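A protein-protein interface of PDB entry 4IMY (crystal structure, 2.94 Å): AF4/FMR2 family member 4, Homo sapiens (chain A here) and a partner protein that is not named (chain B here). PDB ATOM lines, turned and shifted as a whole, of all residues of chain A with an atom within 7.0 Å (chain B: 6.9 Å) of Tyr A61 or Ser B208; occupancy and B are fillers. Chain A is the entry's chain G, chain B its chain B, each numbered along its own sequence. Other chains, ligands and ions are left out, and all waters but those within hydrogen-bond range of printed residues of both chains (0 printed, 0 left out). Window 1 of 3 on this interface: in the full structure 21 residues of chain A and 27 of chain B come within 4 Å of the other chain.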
ATOM      1  N   LYS A  42      19.836  18.943  12.466  1.00  0.00           N
ATOM      2  CA  LYS A  42      19.176  18.749  13.752  1.00  0.00           C
ATOM      3  C   LYS A  42      19.730  17.515  14.454  1.00  0.00           C
ATOM      4  O   LYS A  42      19.556  16.396  13.983  1.00  0.00           O
ATOM      5  CB  LYS A  42      17.663  18.608  13.567  1.00  0.00           C
ATOM      6  CG  LYS A  42      16.949  19.904  13.196  1.00  0.00           C
ATOM      7  CD  LYS A  42      16.658  20.769  14.418  1.00  0.00           C
ATOM      8  CE  LYS A  42      15.511  21.730  14.143  1.00  0.00           C
ATOM      9  NZ  LYS A  42      15.173  22.585  15.314  1.00  0.00           N
ATOM     10  N   VAL A  43      20.404  17.729  15.579  1.00  0.00           N
ATOM     11  CA  VAL A  43      20.959  16.630  16.357  1.00  0.00           C
ATOM     12  C   VAL A  43      19.843  15.893  17.077  1.00  0.00           C
ATOM     13  O   VAL A  43      18.803  16.474  17.384  1.00  0.00           O
ATOM     14  CB  VAL A  43      21.964  17.129  17.414  1.00  0.00           C
ATOM     15  CG1 VAL A  43      22.557  15.960  18.188  1.00  0.00           C
ATOM     16  CG2 VAL A  43      23.065  17.926  16.759  1.00  0.00           C
ATOM     17  N   ILE A  54      19.362  24.433  29.451  1.00  0.00           N
ATOM     18  CA  ILE A  54      18.997  25.560  28.600  1.00  0.00           C
ATOM     19  C   ILE A  54      17.506  25.543  28.282  1.00  0.00           C
ATOM     20  O   ILE A  54      16.852  26.586  28.285  1.00  0.00           O
ATOM     21  CB  ILE A  54      19.789  25.541  27.279  1.00  0.00           C
ATOM     22  CG1 ILE A  54      21.282  25.719  27.551  1.00  0.00           C
ATOM     23  CG2 ILE A  54      19.313  26.648  26.357  1.00  0.00           C
ATOM     24  CD1 ILE A  54      22.172  25.292  26.404  1.00  0.00           C
ATOM     25  N   GLN A  55      16.973  24.355  28.008  1.00  0.00           N
ATOM     26  CA  GLN A  55      15.561  24.209  27.670  1.00  0.00           C
ATOM     27  C   GLN A  55      14.666  24.715  28.801  1.00  0.00           C
ATOM     28  O   GLN A  55      13.497  25.031  28.583  1.00  0.00           O
ATOM     29  CB  GLN A  55      15.235  22.747  27.355  1.00  0.00           C
ATOM     30  N   LEU A  58      15.520  29.007  29.318  1.00  0.00           N
ATOM     31  CA  LEU A  58      14.985  29.856  28.255  1.00  0.00           C
ATOM     32  C   LEU A  58      13.587  29.429  27.804  1.00  0.00           C
ATOM     33  O   LEU A  58      12.897  30.184  27.117  1.00  0.00           O
ATOM     34  CB  LEU A  58      15.919  29.830  27.045  1.00  0.00           C
ATOM     35  CG  LEU A  58      17.400  30.062  27.342  1.00  0.00           C
ATOM     36  CD1 LEU A  58      18.225  29.955  26.069  1.00  0.00           C
ATOM     37  CD2 LEU A  58      17.614  31.412  28.006  1.00  0.00           C
ATOM     38  N   GLY A  59      13.172  28.225  28.187  1.00  0.00           N
ATOM     39  CA  GLY A  59      11.913  27.671  27.726  1.00  0.00           C
ATOM     40  C   GLY A  59      12.138  26.766  26.532  1.00  0.00           C
ATOM     41  O   GLY A  59      13.259  26.663  26.036  1.00  0.00           O
ATOM     42  N   ASN A  60      11.081  26.104  26.070  1.00  0.00           N
ATOM     43  CA  ASN A  60      11.192  25.204  24.925  1.00  0.00           C
ATOM     44  C   ASN A  60      11.431  25.985  23.637  1.00  0.00           C
ATOM     45  O   ASN A  60      10.765  26.986  23.377  1.00  0.00           O
ATOM     46  CB  ASN A  60       9.933  24.344  24.797  1.00  0.00           C
ATOM     47  CG  ASN A  60      10.058  23.282  23.717  1.00  0.00           C
ATOM     48  OD1 ASN A  60      10.624  23.525  22.651  1.00  0.00           O
ATOM     49  ND2 ASN A  60       9.531  22.094  23.993  1.00  0.00           N
ATOM     50  N   TYR A  61      12.380  25.524  22.829  1.00  0.00           N
ATOM     51  CA  TYR A  61      12.747  26.237  21.611  1.00  0.00           C
ATOM     52  C   TYR A  61      11.627  26.229  20.578  1.00  0.00           C
ATOM     53  O   TYR A  61      11.257  27.275  20.049  1.00  0.00           O
ATOM     54  CB  TYR A  61      14.006  25.637  20.991  1.00  0.00           C
ATOM     55  CG  TYR A  61      14.459  26.370  19.750  1.00  0.00           C
ATOM     56  CD1 TYR A  61      15.152  27.569  19.846  1.00  0.00           C
ATOM     57  CD2 TYR A  61      14.188  25.870  18.485  1.00  0.00           C
ATOM     58  CE1 TYR A  61      15.567  28.247  18.721  1.00  0.00           C
ATOM     59  CE2 TYR A  61      14.599  26.542  17.351  1.00  0.00           C
ATOM     60  CZ  TYR A  61      15.290  27.732  17.477  1.00  0.00           C
ATOM     61  OH  TYR A  61      15.708  28.411  16.355  1.00  0.00           O
ATOM     62  N   ASP A  62      11.093  25.048  20.289  1.00  0.00           N
ATOM     63  CA  ASP A  62      10.050  24.910  19.279  1.00  0.00           C
ATOM     64  C   ASP A  62       8.825  25.770  19.594  1.00  0.00           C
ATOM     65  O   ASP A  62       8.083  26.152  18.690  1.00  0.00           O
ATOM     66  CB  ASP A  62       9.642  23.443  19.137  1.00  0.00           C
ATOM     67  CG  ASP A  62      10.733  22.593  18.507  1.00  0.00           C
ATOM     68  OD1 ASP A  62      11.524  23.133  17.702  1.00  0.00           O
ATOM     69  OD2 ASP A  62      10.797  21.383  18.816  1.00  0.00           O
ATOM     70  N   GLU A  63       8.619  26.071  20.872  1.00  0.00           N
ATOM     71  CA  GLU A  63       7.502  26.914  21.288  1.00  0.00           C
ATOM     72  C   GLU A  63       7.839  28.395  21.131  1.00  0.00           C
ATOM     73  O   GLU A  63       7.112  29.141  20.473  1.00  0.00           O
ATOM     74  CB  GLU A  63       7.126  26.627  22.745  1.00  0.00           C
ATOM     75  CG  GLU A  63       6.575  25.229  22.989  1.00  0.00           C
ATOM     76  CD  GLU A  63       6.179  25.004  24.438  1.00  0.00           C
ATOM     77  OE1 GLU A  63       6.265  25.962  25.236  1.00  0.00           O
ATOM     78  OE2 GLU A  63       5.782  23.869  24.778  1.00  0.00           O
ATOM     79  N   MET A  64       8.946  28.813  21.736  1.00  0.00           N
ATOM     80  CA  MET A  64       9.342  30.218  21.738  1.00  0.00           C
ATOM     81  C   MET A  64       9.986  30.632  20.414  1.00  0.00           C
ATOM     82  O   MET A  64      10.234  31.815  20.182  1.00  0.00           O
ATOM     83  CB  MET A  64      10.321  30.485  22.884  1.00  0.00           C
ATOM     84  CG  MET A  64       9.869  29.958  24.237  1.00  0.00           C
ATOM     85  SD  MET A  64       8.181  30.425  24.632  1.00  0.00           S
ATOM     86  CE  MET A  64       8.294  32.201  24.491  1.00  0.00           C
ATOM     87  N   LYS A  65      10.251  29.657  19.551  1.00  0.00           N
ATOM     88  CA  LYS A  65      10.952  29.902  18.291  1.00  0.00           C
ATOM     89  C   LYS A  65      10.321  31.012  17.451  1.00  0.00           C
ATOM     90  O   LYS A  65      11.025  31.859  16.902  1.00  0.00           O
ATOM     91  CB  LYS A  65      11.013  28.609  17.473  1.00  0.00           C
ATOM     92  CG  LYS A  65      11.308  28.808  15.996  1.00  0.00           C
ATOM     93  CD  LYS A  65      11.486  27.475  15.283  1.00  0.00           C
ATOM     94  CE  LYS A  65      10.321  26.535  15.552  1.00  0.00           C
ATOM     95  NZ  LYS A  65      10.468  25.237  14.838  1.00  0.00           N
ATOM     96  N   ASP A  66       8.994  31.006  17.355  1.00  0.00           N
ATOM     97  CA  ASP A  66       8.290  31.929  16.466  1.00  0.00           C
ATOM     98  C   ASP A  66       8.238  33.366  16.992  1.00  0.00           C
ATOM     99  O   ASP A  66       7.644  34.238  16.355  1.00  0.00           O
ATOM    100  CB  ASP A  66       6.868  31.423  16.195  1.00  0.00           C
ATOM    101  CG  ASP A  66       6.843  30.228  15.256  1.00  0.00           C
ATOM    102  OD1 ASP A  66       7.824  30.031  14.505  1.00  0.00           O
ATOM    103  OD2 ASP A  66       5.835  29.489  15.265  1.00  0.00           O
ATOM    104  N   ILE A  68      11.303  34.753  18.455  1.00  0.00           N
ATOM    105  CA  ILE A  68      12.672  35.218  18.276  1.00  0.00           C
ATOM    106  C   ILE A  68      12.812  36.086  17.027  1.00  0.00           C
ATOM    107  O   ILE A  68      12.053  35.944  16.066  1.00  0.00           O
ATOM    108  CB  ILE A  68      13.634  34.021  18.180  1.00  0.00           C
ATOM    109  CG1 ILE A  68      13.711  33.301  19.530  1.00  0.00           C
ATOM    110  CG2 ILE A  68      15.016  34.470  17.746  1.00  0.00           C
ATOM    111  CD1 ILE A  68      14.364  31.937  19.462  1.00  0.00           C
ATOM    112  N   SER B 167      20.306  28.575   8.965  1.00  0.00           N
ATOM    113  CA  SER B 167      18.956  28.946   8.563  1.00  0.00           C
ATOM    114  C   SER B 167      18.529  30.208   9.300  1.00  0.00           C
ATOM    115  O   SER B 167      19.085  30.526  10.348  1.00  0.00           O
ATOM    116  CB  SER B 167      17.989  27.812   8.889  1.00  0.00           C
ATOM    117  OG  SER B 167      18.153  27.387  10.230  1.00  0.00           O
ATOM    118  N   LYS B 168      17.555  30.931   8.753  1.00  0.00           N
ATOM    119  CA  LYS B 168      17.015  32.104   9.437  1.00  0.00           C
ATOM    120  C   LYS B 168      16.738  31.697  10.871  1.00  0.00           C
ATOM    121  O   LYS B 168      17.095  32.396  11.816  1.00  0.00           O
ATOM    122  CB  LYS B 168      15.716  32.589   8.785  1.00  0.00           C
ATOM    123  CG  LYS B 168      15.818  32.872   7.292  1.00  0.00           C
ATOM    124  CD  LYS B 168      14.510  33.415   6.729  1.00  0.00           C
ATOM    125  CE  LYS B 168      14.169  34.788   7.298  1.00  0.00           C
ATOM    126  NZ  LYS B 168      13.211  34.730   8.442  1.00  0.00           N
ATOM    127  N   ASP B 169      16.101  30.539  11.008  1.00  0.00           N
ATOM    128  CA  ASP B 169      15.817  29.932  12.300  1.00  0.00           C
ATOM    129  C   ASP B 169      16.986  30.115  13.264  1.00  0.00           C
ATOM    130  O   ASP B 169      16.847  30.732  14.316  1.00  0.00           O
ATOM    131  CB  ASP B 169      15.534  28.440  12.092  1.00  0.00           C
ATOM    132  CG  ASP B 169      15.017  27.760  13.339  1.00  0.00           C
ATOM    133  OD1 ASP B 169      14.316  28.423  14.132  1.00  0.00           O
ATOM    134  OD2 ASP B 169      15.305  26.557  13.521  1.00  0.00           O
ATOM    135  N   LEU B 170      18.143  29.585  12.884  1.00  0.00           N
ATOM    136  CA  LEU B 170      19.313  29.582  13.755  1.00  0.00           C
ATOM    137  C   LEU B 170      19.999  30.946  13.806  1.00  0.00           C
ATOM    138  O   LEU B 170      20.468  31.375  14.861  1.00  0.00           O
ATOM    139  CB  LEU B 170      20.307  28.515  13.284  1.00  0.00           C
ATOM    140  CG  LEU B 170      21.616  28.401  14.069  1.00  0.00           C
ATOM    141  CD1 LEU B 170      21.354  28.030  15.522  1.00  0.00           C
ATOM    142  CD2 LEU B 170      22.545  27.390  13.415  1.00  0.00           C
ATOM    143  N   ALA B 171      20.056  31.623  12.663  1.00  0.00           N
ATOM    144  CA  ALA B 171      20.733  32.911  12.563  1.00  0.00           C
ATOM    145  C   ALA B 171      20.050  33.949  13.446  1.00  0.00           C
ATOM    146  O   ALA B 171      20.705  34.685  14.188  1.00  0.00           O
ATOM    147  CB  ALA B 171      20.753  33.380  11.117  1.00  0.00           C
ATOM    148  N   GLN B 172      18.726  33.993  13.360  1.00  0.00           N
ATOM    149  CA  GLN B 172      17.939  34.962  14.104  1.00  0.00           C
ATOM    150  C   GLN B 172      18.024  34.688  15.605  1.00  0.00           C
ATOM    151  O   GLN B 172      17.995  35.614  16.414  1.00  0.00           O
ATOM    152  CB  GLN B 172      16.486  34.917  13.633  1.00  0.00           C
ATOM    153  CG  GLN B 172      15.841  36.283  13.496  1.00  0.00           C
ATOM    154  CD  GLN B 172      14.605  36.250  12.624  1.00  0.00           C
ATOM    155  OE1 GLN B 172      14.355  35.267  11.924  1.00  0.00           O
ATOM    156  NE2 GLN B 172      13.824  37.325  12.660  1.00  0.00           N
ATOM    157  N   THR B 173      18.136  33.416  15.968  1.00  0.00           N
ATOM    158  CA  THR B 173      18.230  33.028  17.370  1.00  0.00           C
ATOM    159  C   THR B 173      19.571  33.435  17.962  1.00  0.00           C
ATOM    160  O   THR B 173      19.633  33.906  19.096  1.00  0.00           O
ATOM    161  CB  THR B 173      18.042  31.510  17.550  1.00  0.00           C
ATOM    162  OG1 THR B 173      16.743  31.130  17.081  1.00  0.00           O
ATOM    163  CG2 THR B 173      18.181  31.120  19.018  1.00  0.00           C
ATOM    164  N   LEU B 203      25.231  28.704  22.067  1.00  0.00           N
ATOM    165  CA  LEU B 203      24.046  28.615  22.907  1.00  0.00           C
ATOM    166  C   LEU B 203      22.797  28.405  22.055  1.00  0.00           C
ATOM    167  O   LEU B 203      22.016  27.486  22.298  1.00  0.00           O
ATOM    168  CB  LEU B 203      23.914  29.880  23.757  1.00  0.00           C
ATOM    169  CG  LEU B 203      22.691  29.992  24.667  1.00  0.00           C
ATOM    170  CD1 LEU B 203      22.372  28.667  25.334  1.00  0.00           C
ATOM    171  CD2 LEU B 203      22.940  31.054  25.718  1.00  0.00           C
ATOM    172  N   ALA B 204      22.618  29.255  21.050  1.00  0.00           N
ATOM    173  CA  ALA B 204      21.476  29.141  20.152  1.00  0.00           C
ATOM    174  C   ALA B 204      21.427  27.750  19.529  1.00  0.00           C
ATOM    175  O   ALA B 204      20.348  27.207  19.291  1.00  0.00           O
ATOM    176  CB  ALA B 204      21.544  30.209  19.071  1.00  0.00           C
ATOM    177  N   CYS B 205      22.599  27.174  19.271  1.00  0.00           N
ATOM    178  CA  CYS B 205      22.678  25.843  18.677  1.00  0.00           C
ATOM    179  C   CYS B 205      22.146  24.784  19.634  1.00  0.00           C
ATOM    180  O   CYS B 205      21.319  23.952  19.253  1.00  0.00           O
ATOM    181  CB  CYS B 205      24.116  25.505  18.281  1.00  0.00           C
ATOM    182  SG  CYS B 205      24.668  26.276  16.745  1.00  0.00           S
ATOM    183  N   LYS B 206      22.627  24.813  20.872  1.00  0.00           N
ATOM    184  CA  LYS B 206      22.193  23.851  21.880  1.00  0.00           C
ATOM    185  C   LYS B 206      20.687  23.947  22.101  1.00  0.00           C
ATOM    186  O   LYS B 206      19.984  22.935  22.112  1.00  0.00           O
ATOM    187  CB  LYS B 206      22.925  24.090  23.200  1.00  0.00           C
ATOM    188  CG  LYS B 206      24.416  23.797  23.151  1.00  0.00           C
ATOM    189  CD  LYS B 206      24.692  22.319  22.938  1.00  0.00           C
ATOM    190  CE  LYS B 206      26.183  22.023  22.988  1.00  0.00           C
ATOM    191  NZ  LYS B 206      26.467  20.574  22.783  1.00  0.00           N
ATOM    192  N   TRP B 207      20.199  25.170  22.279  1.00  0.00           N
ATOM    193  CA  TRP B 207      18.778  25.407  22.490  1.00  0.00           C
ATOM    194  C   TRP B 207      17.970  24.917  21.292  1.00  0.00           C
ATOM    195  O   TRP B 207      16.938  24.260  21.447  1.00  0.00           O
ATOM    196  CB  TRP B 207      18.525  26.902  22.708  1.00  0.00           C
ATOM    197  CG  TRP B 207      17.113  27.224  23.093  1.00  0.00           C
ATOM    198  CD1 TRP B 207      16.216  26.389  23.694  1.00  0.00           C
ATOM    199  CD2 TRP B 207      16.431  28.469  22.897  1.00  0.00           C
ATOM    200  NE1 TRP B 207      15.020  27.037  23.887  1.00  0.00           N
ATOM    201  CE2 TRP B 207      15.125  28.315  23.406  1.00  0.00           C
ATOM    202  CE3 TRP B 207      16.795  29.697  22.337  1.00  0.00           C
ATOM    203  CZ2 TRP B 207      14.185  29.341  23.374  1.00  0.00           C
ATOM    204  CZ3 TRP B 207      15.860  30.717  22.308  1.00  0.00           C
ATOM    205  CH2 TRP B 207      14.570  30.533  22.824  1.00  0.00           C
ATOM    206  N   SER B 208      18.458  25.234  20.097  1.00  0.00           N
ATOM    207  CA  SER B 208      17.718  24.980  18.870  1.00  0.00           C
ATOM    208  C   SER B 208      17.952  23.572  18.339  1.00  0.00           C
ATOM    209  O   SER B 208      17.287  23.139  17.396  1.00  0.00           O
ATOM    210  CB  SER B 208      18.118  26.007  17.811  1.00  0.00           C
ATOM    211  OG  SER B 208      17.292  25.903  16.669  1.00  0.00           O
ATOM    212  N   ASN B 209      18.900  22.863  18.945  1.00  0.00           N
ATOM    213  CA  ASN B 209      19.224  21.494  18.544  1.00  0.00           C
ATOM    214  C   ASN B 209      19.911  21.393  17.181  1.00  0.00           C
ATOM    215  O   ASN B 209      19.967  20.316  16.593  1.00  0.00           O
ATOM    216  CB  ASN B 209      17.971  20.608  18.565  1.00  0.00           C
ATOM    217  CG  ASN B 209      17.541  20.240  19.974  1.00  0.00           C
ATOM    218  OD1 ASN B 209      18.360  19.829  20.797  1.00  0.00           O
ATOM    219  ND2 ASN B 209      16.251  20.392  20.260  1.00  0.00           N
ATOM    220  N   TRP B 210      20.433  22.507  16.677  1.00  0.00           N
ATOM    221  CA  TRP B 210      21.245  22.474  15.466  1.00  0.00           C
ATOM    222  C   TRP B 210      22.684  22.174  15.853  1.00  0.00           C
ATOM    223  O   TRP B 210      23.137  22.560  16.934  1.00  0.00           O
ATOM    224  CB  TRP B 210      21.203  23.811  14.720  1.00  0.00           C
ATOM    225  CG  TRP B 210      19.864  24.192  14.165  1.00  0.00           C
ATOM    226  CD1 TRP B 210      19.031  25.157  14.644  1.00  0.00           C
ATOM    227  CD2 TRP B 210      19.211  23.630  13.021  1.00  0.00           C
ATOM    228  NE1 TRP B 210      17.894  25.230  13.874  1.00  0.00           N
ATOM    229  CE2 TRP B 210      17.981  24.300  12.871  1.00  0.00           C
ATOM    230  CE3 TRP B 210      19.544  22.620  12.112  1.00  0.00           C
ATOM    231  CZ2 TRP B 210      17.084  23.998  11.850  1.00  0.00           C
ATOM    232  CZ3 TRP B 210      18.652  22.321  11.099  1.00  0.00           C
ATOM    233  CH2 TRP B 210      17.436  23.005  10.977  1.00  0.00           C
ATOM    234  N   GLU B 211      23.404  21.491  14.969  1.00  0.00           N
ATOM    235  CA  GLU B 211      24.829  21.263  15.171  1.00  0.00           C
ATOM    236  C   GLU B 211      25.622  21.655  13.931  1.00  0.00           C
ATOM    237  O   GLU B 211      25.345  21.187  12.827  1.00  0.00           O
ATOM    238  CB  GLU B 211      25.094  19.806  15.540  1.00  0.00           C
ATOM    239  CG  GLU B 211      26.567  19.456  15.668  1.00  0.00           C
ATOM    240  CD  GLU B 211      26.789  18.167  16.428  1.00  0.00           C
ATOM    241  OE1 GLU B 211      26.304  18.067  17.576  1.00  0.00           O
ATOM    242  OE2 GLU B 211      27.440  17.253  15.879  1.00  0.00           O
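The side-chain hydroxyl of Thr B173 sits at hydrogen-bond distance from the side-chain hydroxyl of Tyr A61. O of Gly A59 sits at hydrogen-bond distance from NE1 of Trp B207, at 2.8 Å. OD1 of Asp B169 lies within hydrogen-bond range of OH of Tyr A61 (2.6 Å). The indole nitrogen (NE1) of Trp B207 lies close to the backbone NH (N) of Tyr A61, at 3.2 Å. The side-chain amino group (NZ) of Lys A42 sits at hydrogen-bond distance from the backbone carbonyl oxygen (O) of Ser B208 (3.0 Å). The side-chain hydroxyl (OG) of Ser B208 lies close to the side-chain hydroxyl (OH) of Tyr A61, at 3.0 Å. The backbone NH of Val A43 sits at hydrogen-bond distance from the backbone carbonyl oxygen of Asn B209 (2.8 Å).
The side-chain carboxylate (OD2) of Asp B169 sits at hydrogen-bond distance from the indole nitrogen (NE1) of Trp B210, at 2.9 Å. OG of Ser B208 lies close to NE1 of Trp B210 (2.9 Å). The backbone NH (N) of Asp A62 is in hydrogen-bond range of the side-chain amide oxygen (OD1) of Asn A60, at 2.8 Å. The backbone carbonyl oxygen (O) of Cys B205 sits at hydrogen-bond distance from the backbone NH (N) of Trp B210 (3.1 Å). OD1 of Asp A62 is in salt-bridge range of NZ of Lys A65 (3.7 Å). The backbone carbonyl oxygen (O) of Asp B169 is in hydrogen-bond range of the side-chain hydroxyl (OG1) of Thr B173.
Among the printed residues, pairs that only touch across the chains: Lys A42 with Asn B209 (3.3 Å), Lys A42 with Trp B210 (3.6 Å), Val A43 with Glu B211 (3.0 Å), Ile A54 with Leu B203 (3.5 Å), Ile A54 with Lys B206 (3.5 Å), Ile A54 with Trp B207 (3.7 Å), Leu A58 with Trp B207 (3.9 Å), Asn A60 with Trp B207 (3.7 Å), Lys A65 with Asp B169 (3.2 Å), Ile A68 with Gln B172 (3.5 Å), Ile A68 with Thr B173 (3.5 Å) and Ile A68 with Trp B207 (3.4 Å).
Printed residues of chain B within 4 Å of Lys A42: Ser B208, Asn B209 and Trp B210. Of the printed residues of chain A, Thr B173 touches Tyr A61 and Ile A68. Glu A63 touches none of the printed residues of chain B. Ala B204 touches none of the printed residues of chain A. The nearest residue of chain B that does not touch Tyr A61 is Leu B170 (4.4 Å).
Of the 14 printed residues of chain A, 9 touch a printed residue of chain B. Hydrophobic or aromatic side chains of chain B within 4 Å of the printed part of chain A: Leu B203, Trp B207 and Trp B210.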
